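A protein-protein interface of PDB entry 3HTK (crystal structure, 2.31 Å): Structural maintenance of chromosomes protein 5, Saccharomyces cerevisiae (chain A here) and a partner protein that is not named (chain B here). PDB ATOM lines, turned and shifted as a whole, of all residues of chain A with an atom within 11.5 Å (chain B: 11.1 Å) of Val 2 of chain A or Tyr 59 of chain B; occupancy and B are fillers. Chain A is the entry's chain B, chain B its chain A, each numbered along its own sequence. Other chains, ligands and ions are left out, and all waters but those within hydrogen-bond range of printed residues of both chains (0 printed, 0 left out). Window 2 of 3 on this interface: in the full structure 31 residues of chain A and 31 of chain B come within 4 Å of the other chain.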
ATOM      1  N   ASP A   1     -27.142 -15.579  12.977  1.00  0.00           N
ATOM      2  CA  ASP A   1     -28.537 -15.168  13.309  1.00  0.00           C
ATOM      3  C   ASP A   1     -28.743 -15.128  14.821  1.00  0.00           C
ATOM      4  O   ASP A   1     -29.718 -14.553  15.309  1.00  0.00           O
ATOM      5  CB  ASP A   1     -29.532 -16.135  12.668  1.00  0.00           C
ATOM      6  N   VAL A   2     -27.819 -15.745  15.554  1.00  0.00           N
ATOM      7  CA  VAL A   2     -27.878 -15.788  17.014  1.00  0.00           C
ATOM      8  C   VAL A   2     -27.886 -14.370  17.586  1.00  0.00           C
ATOM      9  O   VAL A   2     -28.069 -14.167  18.786  1.00  0.00           O
ATOM     10  CB  VAL A   2     -26.667 -16.560  17.593  1.00  0.00           C
ATOM     11  CG1 VAL A   2     -26.782 -16.665  19.109  1.00  0.00           C
ATOM     12  CG2 VAL A   2     -26.586 -17.948  16.962  1.00  0.00           C
ATOM     13  N   SER A   3     -27.682 -13.393  16.707  1.00  0.00           N
ATOM     14  CA  SER A   3     -27.668 -11.987  17.086  1.00  0.00           C
ATOM     15  C   SER A   3     -29.089 -11.497  17.360  1.00  0.00           C
ATOM     16  O   SER A   3     -29.287 -10.389  17.859  1.00  0.00           O
ATOM     17  CB  SER A   3     -27.043 -11.154  15.961  1.00  0.00           C
ATOM     18  OG  SER A   3     -27.105  -9.770  16.250  1.00  0.00           O
ATOM     19  N   GLN A   4     -30.073 -12.333  17.034  1.00  0.00           N
ATOM     20  CA  GLN A   4     -31.478 -11.989  17.233  1.00  0.00           C
ATOM     21  C   GLN A   4     -31.994 -12.360  18.624  1.00  0.00           C
ATOM     22  O   GLN A   4     -32.757 -11.605  19.230  1.00  0.00           O
ATOM     23  CB  GLN A   4     -32.339 -12.674  16.170  1.00  0.00           C
ATOM     24  CG  GLN A   4     -33.813 -12.319  16.256  1.00  0.00           C
ATOM     25  CD  GLN A   4     -34.052 -10.833  16.106  1.00  0.00           C
ATOM     26  OE1 GLN A   4     -33.748 -10.248  15.065  1.00  0.00           O
ATOM     27  NE2 GLN A   4     -34.595 -10.209  17.147  1.00  0.00           N
ATOM     28  N   LYS A   5     -31.586 -13.522  19.126  1.00  0.00           N
ATOM     29  CA  LYS A   5     -32.018 -13.971  20.444  1.00  0.00           C
ATOM     30  C   LYS A   5     -31.642 -12.946  21.510  1.00  0.00           C
ATOM     31  O   LYS A   5     -32.373 -12.751  22.482  1.00  0.00           O
ATOM     32  CB  LYS A   5     -31.385 -15.324  20.785  1.00  0.00           C
ATOM     33  CG  LYS A   5     -31.759 -16.447  19.829  1.00  0.00           C
ATOM     34  CD  LYS A   5     -31.175 -17.785  20.269  1.00  0.00           C
ATOM     35  CE  LYS A   5     -31.509 -18.885  19.268  1.00  0.00           C
ATOM     36  NZ  LYS A   5     -30.961 -20.213  19.669  1.00  0.00           N
ATOM     37  N   ILE A   6     -30.503 -12.289  21.319  1.00  0.00           N
ATOM     38  CA  ILE A   6     -30.033 -11.285  22.268  1.00  0.00           C
ATOM     39  C   ILE A   6     -30.908 -10.029  22.238  1.00  0.00           C
ATOM     40  O   ILE A   6     -30.849  -9.202  23.145  1.00  0.00           O
ATOM     41  CB  ILE A   6     -28.557 -10.895  21.981  1.00  0.00           C
ATOM     42  CG1 ILE A   6     -27.668 -12.139  22.083  1.00  0.00           C
ATOM     43  CG2 ILE A   6     -28.084  -9.831  22.973  1.00  0.00           C
ATOM     44  CD1 ILE A   6     -26.183 -11.864  21.903  1.00  0.00           C
ATOM     45  N   LYS A   7     -31.731  -9.900  21.201  1.00  0.00           N
ATOM     46  CA  LYS A   7     -32.602  -8.736  21.073  1.00  0.00           C
ATOM     47  C   LYS A   7     -34.012  -9.005  21.601  1.00  0.00           C
ATOM     48  O   LYS A   7     -34.638  -8.120  22.190  1.00  0.00           O
ATOM     49  CB  LYS A   7     -32.677  -8.289  19.610  1.00  0.00           C
ATOM     50  CG  LYS A   7     -33.306  -6.917  19.408  1.00  0.00           C
ATOM     51  CD  LYS A   7     -32.473  -5.837  20.076  1.00  0.00           C
ATOM     52  CE  LYS A   7     -33.067  -4.457  19.853  1.00  0.00           C
ATOM     53  NZ  LYS A   7     -32.273  -3.404  20.547  1.00  0.00           N
ATOM     54  N   ASP A   8     -34.514 -10.220  21.384  1.00  0.00           N
ATOM     55  CA  ASP A   8     -35.852 -10.585  21.856  1.00  0.00           C
ATOM     56  C   ASP A   8     -35.853 -10.671  23.378  1.00  0.00           C
ATOM     57  O   ASP A   8     -36.738 -10.136  24.048  1.00  0.00           O
ATOM     58  CB  ASP A   8     -36.281 -11.931  21.272  1.00  0.00           C
ATOM     59  CG  ASP A   8     -36.310 -11.922  19.764  1.00  0.00           C
ATOM     60  OD1 ASP A   8     -36.817 -10.930  19.200  1.00  0.00           O
ATOM     61  OD2 ASP A   8     -35.839 -12.902  19.146  1.00  0.00           O
ATOM     62  N   ILE A   9     -34.843 -11.353  23.908  1.00  0.00           N
ATOM     63  CA  ILE A   9     -34.685 -11.521  25.341  1.00  0.00           C
ATOM     64  C   ILE A   9     -34.338 -10.170  25.971  1.00  0.00           C
ATOM     65  O   ILE A   9     -34.597  -9.946  27.151  1.00  0.00           O
ATOM     66  CB  ILE A   9     -33.574 -12.551  25.646  1.00  0.00           C
ATOM     67  CG1 ILE A   9     -33.865 -13.854  24.893  1.00  0.00           C
ATOM     68  CG2 ILE A   9     -33.506 -12.833  27.146  1.00  0.00           C
ATOM     69  CD1 ILE A   9     -32.729 -14.854  24.945  1.00  0.00           C
ATOM     70  N   ASP A  10     -33.756  -9.274  25.175  1.00  0.00           N
ATOM     71  CA  ASP A  10     -33.398  -7.938  25.649  1.00  0.00           C
ATOM     72  C   ASP A  10     -34.659  -7.066  25.666  1.00  0.00           C
ATOM     73  O   ASP A  10     -34.745  -6.092  26.418  1.00  0.00           O
ATOM     74  CB  ASP A  10     -32.330  -7.311  24.741  1.00  0.00           C
ATOM     75  CG  ASP A  10     -31.097  -6.842  25.517  1.00  0.00           C
ATOM     76  OD1 ASP A  10     -30.466  -7.675  26.207  1.00  0.00           O
ATOM     77  OD2 ASP A  10     -30.757  -5.639  25.433  1.00  0.00           O
ATOM     78  N   LYS B  51     -33.070 -14.079  35.222  1.00  0.00           N
ATOM     79  CA  LYS B  51     -32.851 -15.252  34.392  1.00  0.00           C
ATOM     80  C   LYS B  51     -32.721 -14.934  32.914  1.00  0.00           C
ATOM     81  O   LYS B  51     -31.835 -15.472  32.247  1.00  0.00           O
ATOM     82  CB  LYS B  51     -33.955 -16.288  34.622  1.00  0.00           C
ATOM     83  CG  LYS B  51     -33.937 -16.864  36.029  1.00  0.00           C
ATOM     84  CD  LYS B  51     -32.522 -17.278  36.429  1.00  0.00           C
ATOM     85  CE  LYS B  51     -32.431 -17.629  37.903  1.00  0.00           C
ATOM     86  NZ  LYS B  51     -31.023 -17.897  38.305  1.00  0.00           N
ATOM     87  N   LYS B  52     -33.593 -14.077  32.391  1.00  0.00           N
ATOM     88  CA  LYS B  52     -33.504 -13.708  30.979  1.00  0.00           C
ATOM     89  C   LYS B  52     -32.127 -13.092  30.754  1.00  0.00           C
ATOM     90  O   LYS B  52     -31.528 -13.235  29.688  1.00  0.00           O
ATOM     91  CB  LYS B  52     -34.577 -12.686  30.602  1.00  0.00           C
ATOM     92  CG  LYS B  52     -35.976 -13.233  30.546  1.00  0.00           C
ATOM     93  CD  LYS B  52     -36.064 -14.395  29.588  1.00  0.00           C
ATOM     94  CE  LYS B  52     -37.496 -14.883  29.471  1.00  0.00           C
ATOM     95  NZ  LYS B  52     -38.390 -13.814  28.955  1.00  0.00           N
ATOM     96  N   LYS B  53     -31.643 -12.396  31.778  1.00  0.00           N
ATOM     97  CA  LYS B  53     -30.342 -11.756  31.735  1.00  0.00           C
ATOM     98  C   LYS B  53     -29.276 -12.836  31.551  1.00  0.00           C
ATOM     99  O   LYS B  53     -28.642 -12.920  30.498  1.00  0.00           O
ATOM    100  CB  LYS B  53     -30.097 -10.991  33.039  1.00  0.00           C
ATOM    101  CG  LYS B  53     -28.713 -10.385  33.172  1.00  0.00           C
ATOM    102  CD  LYS B  53     -28.502  -9.212  32.223  1.00  0.00           C
ATOM    103  CE  LYS B  53     -29.332  -7.997  32.626  1.00  0.00           C
ATOM    104  NZ  LYS B  53     -30.792  -8.254  32.551  1.00  0.00           N
ATOM    105  N   ASN B  54     -29.095 -13.663  32.581  1.00  0.00           N
ATOM    106  CA  ASN B  54     -28.118 -14.748  32.555  1.00  0.00           C
ATOM    107  C   ASN B  54     -28.119 -15.492  31.225  1.00  0.00           C
ATOM    108  O   ASN B  54     -27.087 -16.019  30.808  1.00  0.00           O
ATOM    109  CB  ASN B  54     -28.385 -15.730  33.696  1.00  0.00           C
ATOM    110  CG  ASN B  54     -27.974 -15.177  35.050  1.00  0.00           C
ATOM    111  OD1 ASN B  54     -28.136 -15.836  36.078  1.00  0.00           O
ATOM    112  ND2 ASN B  54     -27.433 -13.961  35.058  1.00  0.00           N
ATOM    113  N   GLN B  55     -29.274 -15.540  30.569  1.00  0.00           N
ATOM    114  CA  GLN B  55     -29.381 -16.202  29.277  1.00  0.00           C
ATOM    115  C   GLN B  55     -28.559 -15.452  28.225  1.00  0.00           C
ATOM    116  O   GLN B  55     -27.783 -16.055  27.483  1.00  0.00           O
ATOM    117  CB  GLN B  55     -30.846 -16.279  28.844  1.00  0.00           C
ATOM    118  CG  GLN B  55     -31.648 -17.331  29.597  1.00  0.00           C
ATOM    119  CD  GLN B  55     -33.106 -17.372  29.175  1.00  0.00           C
ATOM    120  OE1 GLN B  55     -33.423 -17.343  27.981  1.00  0.00           O
ATOM    121  NE2 GLN B  55     -34.005 -17.453  30.155  1.00  0.00           N
ATOM    122  N   ASN B  56     -28.737 -14.134  28.168  1.00  0.00           N
ATOM    123  CA  ASN B  56     -28.008 -13.288  27.225  1.00  0.00           C
ATOM    124  C   ASN B  56     -26.542 -13.207  27.608  1.00  0.00           C
ATOM    125  O   ASN B  56     -25.678 -12.997  26.760  1.00  0.00           O
ATOM    126  CB  ASN B  56     -28.607 -11.884  27.204  1.00  0.00           C
ATOM    127  CG  ASN B  56     -29.714 -11.753  26.204  1.00  0.00           C
ATOM    128  OD1 ASN B  56     -30.432 -12.719  25.929  1.00  0.00           O
ATOM    129  ND2 ASN B  56     -29.874 -10.557  25.652  1.00  0.00           N
ATOM    130  N   GLU B  57     -26.276 -13.356  28.900  1.00  0.00           N
ATOM    131  CA  GLU B  57     -24.916 -13.333  29.415  1.00  0.00           C
ATOM    132  C   GLU B  57     -24.205 -14.464  28.668  1.00  0.00           C
ATOM    133  O   GLU B  57     -23.029 -14.362  28.309  1.00  0.00           O
ATOM    134  CB  GLU B  57     -24.954 -13.605  30.922  1.00  0.00           C
ATOM    135  CG  GLU B  57     -23.661 -13.368  31.677  1.00  0.00           C
ATOM    136  CD  GLU B  57     -23.867 -13.425  33.183  1.00  0.00           C
ATOM    137  OE1 GLU B  57     -24.616 -12.575  33.711  1.00  0.00           O
ATOM    138  OE2 GLU B  57     -23.292 -14.317  33.841  1.00  0.00           O
ATOM    139  N   TYR B  58     -24.962 -15.529  28.419  1.00  0.00           N
ATOM    140  CA  TYR B  58     -24.495 -16.714  27.712  1.00  0.00           C
ATOM    141  C   TYR B  58     -24.581 -16.512  26.188  1.00  0.00           C
ATOM    142  O   TYR B  58     -24.137 -17.359  25.414  1.00  0.00           O
ATOM    143  CB  TYR B  58     -25.337 -17.915  28.163  1.00  0.00           C
ATOM    144  CG  TYR B  58     -25.291 -19.120  27.253  1.00  0.00           C
ATOM    145  CD1 TYR B  58     -24.153 -19.925  27.175  1.00  0.00           C
ATOM    146  CD2 TYR B  58     -26.390 -19.450  26.460  1.00  0.00           C
ATOM    147  CE1 TYR B  58     -24.113 -21.033  26.324  1.00  0.00           C
ATOM    148  CE2 TYR B  58     -26.364 -20.548  25.610  1.00  0.00           C
ATOM    149  CZ  TYR B  58     -25.227 -21.336  25.545  1.00  0.00           C
ATOM    150  OH  TYR B  58     -25.216 -22.425  24.702  1.00  0.00           O
ATOM    151  N   TYR B  59     -25.151 -15.381  25.776  1.00  0.00           N
ATOM    152  CA  TYR B  59     -25.307 -14.997  24.364  1.00  0.00           C
ATOM    153  C   TYR B  59     -26.443 -15.689  23.600  1.00  0.00           C
ATOM    154  O   TYR B  59     -26.483 -15.625  22.371  1.00  0.00           O
ATOM    155  CB  TYR B  59     -23.998 -15.214  23.584  1.00  0.00           C
ATOM    156  CG  TYR B  59     -22.735 -14.855  24.338  1.00  0.00           C
ATOM    157  CD1 TYR B  59     -22.505 -13.553  24.787  1.00  0.00           C
ATOM    158  CD2 TYR B  59     -21.773 -15.829  24.619  1.00  0.00           C
ATOM    159  CE1 TYR B  59     -21.345 -13.231  25.500  1.00  0.00           C
ATOM    160  CE2 TYR B  59     -20.616 -15.522  25.329  1.00  0.00           C
ATOM    161  CZ  TYR B  59     -20.407 -14.223  25.768  1.00  0.00           C
ATOM    162  OH  TYR B  59     -19.267 -13.927  26.481  1.00  0.00           O
ATOM    163  N   ARG B  60     -27.369 -16.336  24.303  1.00  0.00           N
ATOM    164  CA  ARG B  60     -28.474 -17.015  23.624  1.00  0.00           C
ATOM    165  C   ARG B  60     -29.623 -17.425  24.544  1.00  0.00           C
ATOM    166  O   ARG B  60     -29.646 -16.977  25.711  1.00  0.00           O
ATOM    167  CB  ARG B  60     -27.952 -18.234  22.882  1.00  0.00           C
ATOM    168  OXT ARG B  60     -30.497 -18.187  24.073  1.00  0.00           O
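ND2 of Asn 56 of chain B lies within hydrogen-bond range of O of Ile 6 of chain A (3.0 Å). ND2 of Asn 56 of chain B is in hydrogen-bond range of OD1 of Asp 10 of chain A (3.0 Å).
The backbone carbonyl oxygen of Gln 55 of chain B is in hydrogen-bond range of the backbone NH of Arg 60 of chain B (3.2 Å).
Among the printed residues, pairs that only touch across the chains: Ile 9 of chain A with Asn 56 of chain B, Ile 9 of chain A with Lys 52 of chain B, Val 2 of chain A with Tyr 59 of chain B, Ile 6 of chain A with Tyr 59 of chain B, Ile 9 of chain A with Arg 60 of chain B, Lys 5 of chain A with Arg 60 of chain B, Lys 5 of chain A with Asn 56 of chain B and Ile 9 of chain A with Gln 55 of chain B.
No residue of chain B comes within 4 Å of Asp 1 of chain A. No residue of chain B comes within 4 Å of Ser 3 of chain A. Of the printed residues of chain B, Lys 5 of chain A touches Asn 56 (3.96 Å) and Arg 60 (3.9 Å). Of the printed residues of chain B, Ile 6 of chain A touches Asn 56 and Tyr 59. Of the printed residues of chain B, Asp 10 of chain A touches Asn 56 (3.0 Å). Of the printed residues of chain A, Lys 52 of chain B touches Ile 9. Of the printed residues of chain A, Gln 55 of chain B touches Ile 9 (3.99 Å). Asn 56 of chain B touches four residues of chain A. The nearest printed residue of chain A that does not touch Lys 52 of chain B is Asp 8 of chain A (6.4 Å).
Printed residues of chain A that touch a printed residue of chain B: Val 2, Lys 5, Ile 6, Ile 9 and Asp 10. Among the printed residues, no Asp or Glu carboxylate lies within 4 Å of a Lys or Arg side-chain nitrogen of the other chain.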
